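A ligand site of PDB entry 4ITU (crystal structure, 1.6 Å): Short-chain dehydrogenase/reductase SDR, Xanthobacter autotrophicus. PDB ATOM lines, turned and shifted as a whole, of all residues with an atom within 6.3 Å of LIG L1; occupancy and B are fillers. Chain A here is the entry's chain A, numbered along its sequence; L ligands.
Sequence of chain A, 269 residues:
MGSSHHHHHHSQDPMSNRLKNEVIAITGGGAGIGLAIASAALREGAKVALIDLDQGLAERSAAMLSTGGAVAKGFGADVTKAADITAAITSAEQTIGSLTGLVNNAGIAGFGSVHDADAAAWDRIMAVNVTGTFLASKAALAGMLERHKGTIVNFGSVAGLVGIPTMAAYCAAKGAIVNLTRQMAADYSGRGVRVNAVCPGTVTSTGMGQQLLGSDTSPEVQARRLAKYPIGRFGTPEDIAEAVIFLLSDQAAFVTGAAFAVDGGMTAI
An oxygen (O1) of LIG L1 lies within hydrogen-bond range of the side-chain hydroxyl of Ser 157, at 2.5 Å. The side-chain hydroxyl of Thr 202 is in hydrogen-bond range of an oxygen (O4) of LIG L1, 2.6 Å away. OH of Tyr 170 sits at hydrogen-bond distance from O1 of LIG L1, 2.7 Å away. The side-chain hydroxyl (OH) of Tyr 229 lies within hydrogen-bond range of an oxygen (O3) of LIG L1. The guanidinium group (NE) of Arg 225 lies within salt-bridge range of an oxygen (O4) of LIG L1 (3.5 Å). The side-chain amino group (NZ) of Lys 228 lies within salt-bridge range of an oxygen (O2) of LIG L1. The side-chain hydroxyl (OH) of Tyr 170 lies within hydrogen-bond range of an oxygen (O13) of LG2 L2. The side-chain sulfur (SD) of Met 208 sits close to an oxygen (O13) of LG2 L2 (3.6 Å). The side-chain amino group (NZ) of Lys 174 lies within hydrogen-bond range of an oxygen (O12) of LG2 L2 (3.0 Å). O14 of LG2 L2 is in hydrogen-bond range of N of Val 203, at 2.8 Å. N7 of LG2 L2 lies within hydrogen-bond range of O of Val 203.
N of Ala 159 lies close to OG of Ser 157. The side-chain hydroxyl (OH) of Tyr 229 is in hydrogen-bond range of the backbone NH (N) of Thr 202 (2.9 Å). N of Val 158 lies within hydrogen-bond range of O of Pro 200, at 2.9 Å.
Val 158 touches LIG L1. Met 208 touches LIG L1 (SD to C1, 3.8 Å). CE of Met 266 touches O3 of LIG L1 (3.6 Å). Hydrophobic or aromatic side chains within 4 Å of LIG L1: Val 158, Tyr 170, Met 208, Tyr 229 and Met 266. Nine residues have an atom within 4 Å of LIG L1: Ser 157, Val 158, Tyr 170, Thr 202, Met 208, Arg 225, Lys 228, Tyr 229 and Met 266.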
ATOM      1  N   ALA A 109     -24.531   7.142   5.601  1.00  0.00           N
ATOM      2  CA  ALA A 109     -23.090   7.241   5.740  1.00  0.00           C
ATOM      3  C   ALA A 109     -22.709   8.720   5.741  1.00  0.00           C
ATOM      4  O   ALA A 109     -23.527   9.585   5.411  1.00  0.00           O
ATOM      5  CB  ALA A 109     -22.393   6.519   4.606  1.00  0.00           C
ATOM      6  N   GLY A 156     -24.495  -4.836   8.279  1.00  0.00           N
ATOM      7  CA  GLY A 156     -23.151  -4.398   8.565  1.00  0.00           C
ATOM      8  C   GLY A 156     -22.557  -3.842   7.283  1.00  0.00           C
ATOM      9  O   GLY A 156     -23.270  -3.270   6.442  1.00  0.00           O
ATOM     10  N   SER A 157     -21.252  -4.007   7.136  1.00  0.00           N
ATOM     11  CA  SER A 157     -20.541  -3.535   5.969  1.00  0.00           C
ATOM     12  C   SER A 157     -19.121  -4.034   6.142  1.00  0.00           C
ATOM     13  O   SER A 157     -18.756  -4.450   7.246  1.00  0.00           O
ATOM     14  CB  SER A 157     -20.546  -2.009   5.903  1.00  0.00           C
ATOM     15  OG  SER A 157     -19.650  -1.532   4.922  1.00  0.00           O
ATOM     16  N   VAL A 158     -18.314  -4.005   5.084  1.00  0.00           N
ATOM     17  CA  VAL A 158     -16.895  -4.174   5.285  1.00  0.00           C
ATOM     18  C   VAL A 158     -16.424  -3.119   6.292  1.00  0.00           C
ATOM     19  O   VAL A 158     -15.524  -3.373   7.099  1.00  0.00           O
ATOM     20  CB  VAL A 158     -16.088  -4.079   3.974  1.00  0.00           C
ATOM     21  CG1 VAL A 158     -16.367  -5.292   3.097  1.00  0.00           C
ATOM     22  CG2 VAL A 158     -16.427  -2.795   3.218  1.00  0.00           C
ATOM     23  N   ALA A 159     -17.101  -1.963   6.308  1.00  0.00           N
ATOM     24  CA  ALA A 159     -16.793  -0.890   7.251  1.00  0.00           C
ATOM     25  C   ALA A 159     -17.118  -1.230   8.713  1.00  0.00           C
ATOM     26  O   ALA A 159     -16.729  -0.481   9.615  1.00  0.00           O
ATOM     27  CB  ALA A 159     -17.502   0.407   6.856  1.00  0.00           C
ATOM     28  N   ILE A 164     -12.048   2.121   7.920  1.00  0.00           N
ATOM     29  CA  ILE A 164     -12.044   2.830   6.654  1.00  0.00           C
ATOM     30  C   ILE A 164     -11.609   4.252   6.906  1.00  0.00           C
ATOM     31  O   ILE A 164     -12.202   4.924   7.743  1.00  0.00           O
ATOM     32  CB  ILE A 164     -13.460   2.864   6.026  1.00  0.00           C
ATOM     33  CG1 ILE A 164     -14.055   1.463   5.926  1.00  0.00           C
ATOM     34  CG2 ILE A 164     -13.431   3.553   4.645  1.00  0.00           C
ATOM     35  CD1 ILE A 164     -13.240   0.488   5.083  1.00  0.00           C
ATOM     36  N   PRO A 165     -10.554   4.722   6.206  1.00  0.00           N
ATOM     37  CA  PRO A 165     -10.092   6.098   6.420  1.00  0.00           C
ATOM     38  C   PRO A 165     -11.219   7.117   6.311  1.00  0.00           C
ATOM     39  O   PRO A 165     -12.070   7.011   5.421  1.00  0.00           O
ATOM     40  CB  PRO A 165      -9.081   6.309   5.282  1.00  0.00           C
ATOM     41  CG  PRO A 165      -8.578   4.943   4.948  1.00  0.00           C
ATOM     42  CD  PRO A 165      -9.717   3.980   5.240  1.00  0.00           C
ATOM     43  N   MET A 167     -13.959   7.668   7.935  1.00  0.00           N
ATOM     44  CA  MET A 167     -15.360   7.350   8.205  1.00  0.00           C
ATOM     45  C   MET A 167     -15.552   6.850   9.626  1.00  0.00           C
ATOM     46  O   MET A 167     -15.999   5.714   9.847  1.00  0.00           O
ATOM     47  CB  MET A 167     -15.876   6.313   7.207  1.00  0.00           C
ATOM     48  CG  MET A 167     -15.791   6.764   5.755  1.00  0.00           C
ATOM     49  SD  MET A 167     -16.601   5.589   4.649  1.00  0.00           S
ATOM     50  CE  MET A 167     -18.326   6.055   4.849  1.00  0.00           C
ATOM     51  N   TYR A 170     -19.362   6.136  10.857  1.00  0.00           N
ATOM     52  CA  TYR A 170     -19.901   5.026  10.079  1.00  0.00           C
ATOM     53  C   TYR A 170     -19.246   3.695  10.473  1.00  0.00           C
ATOM     54  O   TYR A 170     -19.951   2.685  10.636  1.00  0.00           O
ATOM     55  CB  TYR A 170     -19.761   5.307   8.570  1.00  0.00           C
ATOM     56  CG  TYR A 170     -20.469   4.307   7.675  1.00  0.00           C
ATOM     57  CD1 TYR A 170     -21.855   4.317   7.530  1.00  0.00           C
ATOM     58  CD2 TYR A 170     -19.751   3.361   6.974  1.00  0.00           C
ATOM     59  CE1 TYR A 170     -22.506   3.397   6.705  1.00  0.00           C
ATOM     60  CE2 TYR A 170     -20.381   2.445   6.139  1.00  0.00           C
ATOM     61  CZ  TYR A 170     -21.758   2.469   6.009  1.00  0.00           C
ATOM     62  OH  TYR A 170     -22.358   1.548   5.175  1.00  0.00           O
ATOM     63  N   LYS A 174     -21.412   0.630  12.092  1.00  0.00           N
ATOM     64  CA  LYS A 174     -21.460  -0.687  11.482  1.00  0.00           C
ATOM     65  C   LYS A 174     -20.813  -1.729  12.407  1.00  0.00           C
ATOM     66  O   LYS A 174     -21.263  -2.876  12.447  1.00  0.00           O
ATOM     67  CB  LYS A 174     -20.860  -0.666  10.076  1.00  0.00           C
ATOM     68  CG  LYS A 174     -21.684   0.182   9.082  1.00  0.00           C
ATOM     69  CD  LYS A 174     -23.176  -0.223   9.149  1.00  0.00           C
ATOM     70  CE  LYS A 174     -23.970   0.278   7.961  1.00  0.00           C
ATOM     71  NZ  LYS A 174     -25.404  -0.155   7.993  1.00  0.00           N
ATOM     72  N   PRO A 200     -21.785  -6.097   3.330  1.00  0.00           N
ATOM     73  CA  PRO A 200     -21.436  -5.899   1.928  1.00  0.00           C
ATOM     74  C   PRO A 200     -20.158  -5.097   1.732  1.00  0.00           C
ATOM     75  O   PRO A 200     -19.829  -4.227   2.563  1.00  0.00           O
ATOM     76  CB  PRO A 200     -22.627  -5.081   1.390  1.00  0.00           C
ATOM     77  CG  PRO A 200     -23.731  -5.256   2.426  1.00  0.00           C
ATOM     78  CD  PRO A 200     -23.005  -5.364   3.718  1.00  0.00           C
ATOM     79  N   GLY A 201     -19.442  -5.398   0.654  1.00  0.00           N
ATOM     80  CA  GLY A 201     -18.433  -4.492   0.139  1.00  0.00           C
ATOM     81  C   GLY A 201     -19.112  -3.345  -0.595  1.00  0.00           C
ATOM     82  O   GLY A 201     -20.346  -3.317  -0.714  1.00  0.00           O
ATOM     83  N   THR A 202     -18.318  -2.402  -1.077  1.00  0.00           N
ATOM     84  CA  THR A 202     -18.834  -1.234  -1.815  1.00  0.00           C
ATOM     85  C   THR A 202     -19.754  -1.588  -2.980  1.00  0.00           C
ATOM     86  O   THR A 202     -19.427  -2.451  -3.821  1.00  0.00           O
ATOM     87  CB  THR A 202     -17.664  -0.389  -2.306  1.00  0.00           C
ATOM     88  OG1 THR A 202     -16.996   0.163  -1.178  1.00  0.00           O
ATOM     89  CG2 THR A 202     -18.164   0.748  -3.187  1.00  0.00           C
ATOM     90  N   VAL A 203     -20.898  -0.920  -3.023  1.00  0.00           N
ATOM     91  CA  VAL A 203     -21.861  -1.041  -4.112  1.00  0.00           C
ATOM     92  C   VAL A 203     -22.023   0.369  -4.654  1.00  0.00           C
ATOM     93  O   VAL A 203     -22.630   1.228  -4.003  1.00  0.00           O
ATOM     94  CB  VAL A 203     -23.210  -1.583  -3.601  1.00  0.00           C
ATOM     95  CG1 VAL A 203     -24.231  -1.647  -4.732  1.00  0.00           C
ATOM     96  CG2 VAL A 203     -23.024  -2.975  -2.954  1.00  0.00           C
ATOM     97  N   MET A 208     -25.910   5.909  -1.813  1.00  0.00           N
ATOM     98  CA  MET A 208     -24.792   5.898  -0.880  1.00  0.00           C
ATOM     99  C   MET A 208     -23.495   5.615  -1.623  1.00  0.00           C
ATOM    100  O   MET A 208     -22.459   6.204  -1.318  1.00  0.00           O
ATOM    101  CB  MET A 208     -24.982   4.854   0.223  1.00  0.00           C
ATOM    102  CG  MET A 208     -23.872   4.898   1.264  1.00  0.00           C
ATOM    103  SD  MET A 208     -24.132   3.724   2.603  1.00  0.00           S
ATOM    104  CE  MET A 208     -25.691   4.291   3.263  1.00  0.00           C
ATOM    105  N   LEU A 212     -20.254   7.994  -1.819  1.00  0.00           N
ATOM    106  CA  LEU A 212     -18.882   7.560  -1.530  1.00  0.00           C
ATOM    107  C   LEU A 212     -17.891   7.977  -2.621  1.00  0.00           C
ATOM    108  O   LEU A 212     -16.833   8.520  -2.318  1.00  0.00           O
ATOM    109  CB  LEU A 212     -18.833   6.035  -1.342  1.00  0.00           C
ATOM    110  CG  LEU A 212     -17.453   5.431  -1.073  1.00  0.00           C
ATOM    111  CD1 LEU A 212     -16.886   5.922   0.261  1.00  0.00           C
ATOM    112  CD2 LEU A 212     -17.503   3.893  -1.115  1.00  0.00           C
ATOM    113  N   ARG A 225      -9.117   2.231  -4.573  1.00  0.00           N
ATOM    114  CA  ARG A 225     -10.255   1.597  -3.906  1.00  0.00           C
ATOM    115  C   ARG A 225     -10.593   0.262  -4.562  1.00  0.00           C
ATOM    116  O   ARG A 225     -10.799  -0.729  -3.862  1.00  0.00           O
ATOM    117  CB  ARG A 225     -11.473   2.524  -3.915  1.00  0.00           C
ATOM    118  CG  ARG A 225     -12.683   1.943  -3.208  1.00  0.00           C
ATOM    119  CD  ARG A 225     -13.913   2.866  -3.281  1.00  0.00           C
ATOM    120  NE  ARG A 225     -13.797   4.020  -2.383  1.00  0.00           N
ATOM    121  CZ  ARG A 225     -13.649   5.273  -2.800  1.00  0.00           C
ATOM    122  NH1 ARG A 225     -13.608   5.543  -4.098  1.00  0.00           N
ATOM    123  NH2 ARG A 225     -13.555   6.262  -1.923  1.00  0.00           N
ATOM    124  N   LYS A 228      -8.684  -2.907  -3.736  1.00  0.00           N
ATOM    125  CA  LYS A 228      -8.945  -3.530  -2.446  1.00  0.00           C
ATOM    126  C   LYS A 228      -9.833  -4.765  -2.615  1.00  0.00           C
ATOM    127  O   LYS A 228      -9.975  -5.559  -1.688  1.00  0.00           O
ATOM    128  CB  LYS A 228      -9.628  -2.545  -1.487  1.00  0.00           C
ATOM    129  CG  LYS A 228      -8.790  -1.302  -1.172  1.00  0.00           C
ATOM    130  CD  LYS A 228      -9.466  -0.429  -0.118  1.00  0.00           C
ATOM    131  CE  LYS A 228      -8.584   0.756   0.256  1.00  0.00           C
ATOM    132  NZ  LYS A 228      -9.128   1.521   1.419  1.00  0.00           N
ATOM    133  N   TYR A 229     -10.410  -4.921  -3.803  1.00  0.00           N
ATOM    134  CA  TYR A 229     -11.348  -5.993  -4.090  1.00  0.00           C
ATOM    135  C   TYR A 229     -10.745  -7.046  -5.020  1.00  0.00           C
ATOM    136  O   TYR A 229     -10.606  -6.808  -6.223  1.00  0.00           O
ATOM    137  CB  TYR A 229     -12.630  -5.397  -4.701  1.00  0.00           C
ATOM    138  CG  TYR A 229     -13.404  -4.614  -3.684  1.00  0.00           C
ATOM    139  CD1 TYR A 229     -13.050  -3.305  -3.365  1.00  0.00           C
ATOM    140  CD2 TYR A 229     -14.450  -5.201  -2.970  1.00  0.00           C
ATOM    141  CE1 TYR A 229     -13.735  -2.600  -2.393  1.00  0.00           C
ATOM    142  CE2 TYR A 229     -15.129  -4.505  -1.999  1.00  0.00           C
ATOM    143  CZ  TYR A 229     -14.776  -3.212  -1.718  1.00  0.00           C
ATOM    144  OH  TYR A 229     -15.462  -2.532  -0.749  1.00  0.00           O
ATOM    145  N   PHE A 234     -16.727  -3.831  -8.132  1.00  0.00           N
ATOM    146  CA  PHE A 234     -17.532  -3.523  -6.959  1.00  0.00           C
ATOM    147  C   PHE A 234     -18.820  -4.324  -7.020  1.00  0.00           C
ATOM    148  O   PHE A 234     -19.089  -4.987  -8.019  1.00  0.00           O
ATOM    149  CB  PHE A 234     -17.834  -2.036  -6.877  1.00  0.00           C
ATOM    150  CG  PHE A 234     -16.623  -1.185  -6.660  1.00  0.00           C
ATOM    151  CD1 PHE A 234     -15.847  -1.326  -5.516  1.00  0.00           C
ATOM    152  CD2 PHE A 234     -16.254  -0.245  -7.595  1.00  0.00           C
ATOM    153  CE1 PHE A 234     -14.733  -0.535  -5.304  1.00  0.00           C
ATOM    154  CE2 PHE A 234     -15.130   0.555  -7.398  1.00  0.00           C
ATOM    155  CZ  PHE A 234     -14.366   0.406  -6.254  1.00  0.00           C
ATOM    156  N   MET A 266     -12.815  -8.527  -0.152  1.00  0.00           N
ATOM    157  CA  MET A 266     -12.155  -7.379   0.472  1.00  0.00           C
ATOM    158  C   MET A 266     -11.590  -7.693   1.857  1.00  0.00           C
ATOM    159  O   MET A 266     -10.423  -7.412   2.135  1.00  0.00           O
ATOM    160  CB  MET A 266     -13.117  -6.171   0.529  1.00  0.00           C
ATOM    161  CG  MET A 266     -12.483  -4.843   0.967  1.00  0.00           C
ATOM    162  SD  MET A 266     -12.466  -4.618   2.763  1.00  0.00           S
ATOM    163  CE  MET A 266     -12.070  -2.870   2.899  1.00  0.00           C
HETATM  164  C1  LIG L   1     -20.444   2.774   2.592  1.00  0.00           C
HETATM  165  C2  LIG L   1     -20.121   1.282   2.427  1.00  0.00           C
HETATM  166  O1  LIG L   1     -20.280   0.589   3.671  1.00  0.00           O
HETATM  167  C3  LIG L   1     -18.694   1.150   1.924  1.00  0.00           C
HETATM  168  S1  LIG L   1     -17.538   1.899   3.120  1.00  0.00           S
HETATM  169  C4  LIG L   1     -16.072   1.903   2.048  1.00  0.00           C
HETATM  170  C5  LIG L   1     -15.596   0.504   1.729  1.00  0.00           C
HETATM  171  S2  LIG L   1     -14.166   0.569   0.605  1.00  0.00           S
HETATM  172  O2  LIG L   1     -13.078   1.452   1.149  1.00  0.00           O
HETATM  173  O3  LIG L   1     -13.700  -0.769   0.424  1.00  0.00           O
HETATM  174  O4  LIG L   1     -14.640   1.118  -0.712  1.00  0.00           O
HETATM  175  P1  LG2 L   2     -29.255   4.162  -0.060  1.00  0.00           P
HETATM  176  O1  LG2 L   2     -29.181   4.017  -1.617  1.00  0.00           O
HETATM  177  O2  LG2 L   2     -28.646   5.514   0.364  1.00  0.00           O
HETATM  178  O3  LG2 L   2     -30.758   4.074   0.353  1.00  0.00           O
HETATM  179  C1  LG2 L   2     -31.054   4.125   1.701  1.00  0.00           C
HETATM  180  C2  LG2 L   2     -32.537   4.167   1.901  1.00  0.00           C
HETATM  181  O4  LG2 L   2     -32.720   4.227   3.259  1.00  0.00           O
HETATM  182  C3  LG2 L   2     -33.122   5.391   1.260  1.00  0.00           C
HETATM  183  O5  LG2 L   2     -34.256   5.133   0.524  1.00  0.00           O
HETATM  184  C4  LG2 L   2     -33.397   6.276   2.426  1.00  0.00           C
HETATM  185  O6  LG2 L   2     -34.513   7.087   2.250  1.00  0.00           O
HETATM  186  C5  LG2 L   2     -33.587   5.282   3.520  1.00  0.00           C
HETATM  187  N1  LG2 L   2     -33.388   5.868   4.841  1.00  0.00           N
HETATM  188  C6  LG2 L   2     -32.403   6.706   5.239  1.00  0.00           C
HETATM  189  N2  LG2 L   2     -32.598   7.043   6.506  1.00  0.00           N
HETATM  190  C7  LG2 L   2     -33.707   6.448   6.963  1.00  0.00           C
HETATM  191  C8  LG2 L   2     -34.387   6.430   8.174  1.00  0.00           C
HETATM  192  N3  LG2 L   2     -33.898   7.187   9.276  1.00  0.00           N
HETATM  193  N4  LG2 L   2     -35.493   5.691   8.305  1.00  0.00           N
HETATM  194  C9  LG2 L   2     -35.990   4.971   7.288  1.00  0.00           C
HETATM  195  N5  LG2 L   2     -35.359   4.965   6.097  1.00  0.00           N
HETATM  196  C10 LG2 L   2     -34.223   5.688   5.909  1.00  0.00           C
HETATM  197  O7  LG2 L   2     -28.441   3.034   0.704  1.00  0.00           O
HETATM  198  P2  LG2 L   2     -27.786   1.689   0.159  1.00  0.00           P
HETATM  199  O8  LG2 L   2     -28.805   0.881  -0.642  1.00  0.00           O
HETATM  200  O9  LG2 L   2     -26.497   1.967  -0.645  1.00  0.00           O
HETATM  201  O10 LG2 L   2     -27.386   0.957   1.490  1.00  0.00           O
HETATM  202  C11 LG2 L   2     -28.343   0.227   2.239  1.00  0.00           C
HETATM  203  C12 LG2 L   2     -27.636  -0.382   3.452  1.00  0.00           C
HETATM  204  O11 LG2 L   2     -26.457  -1.071   3.025  1.00  0.00           O
HETATM  205  C13 LG2 L   2     -27.218   0.605   4.504  1.00  0.00           C
HETATM  206  O12 LG2 L   2     -27.389   0.090   5.783  1.00  0.00           O
HETATM  207  C14 LG2 L   2     -25.800   0.812   4.190  1.00  0.00           C
HETATM  208  O13 LG2 L   2     -25.088   1.400   5.221  1.00  0.00           O
HETATM  209  C15 LG2 L   2     -25.368  -0.559   3.781  1.00  0.00           C
HETATM  210  N6  LG2 L   2     -24.197  -0.554   2.897  1.00  0.00           N
HETATM  211  C16 LG2 L   2     -23.981   0.109   1.683  1.00  0.00           C
HETATM  212  C17 LG2 L   2     -22.901  -0.201   0.881  1.00  0.00           C
HETATM  213  C18 LG2 L   2     -22.733   0.583  -0.369  1.00  0.00           C
HETATM  214  O14 LG2 L   2     -21.615   0.664  -0.869  1.00  0.00           O
HETATM  215  N7  LG2 L   2     -23.847   1.260  -0.972  1.00  0.00           N
HETATM  216  C19 LG2 L   2     -21.915  -1.286   1.274  1.00  0.00           C
HETATM  217  C20 LG2 L   2     -22.091  -1.756   2.710  1.00  0.00           C
HETATM  218  C21 LG2 L   2     -23.215  -1.388   3.454  1.00  0.00           C
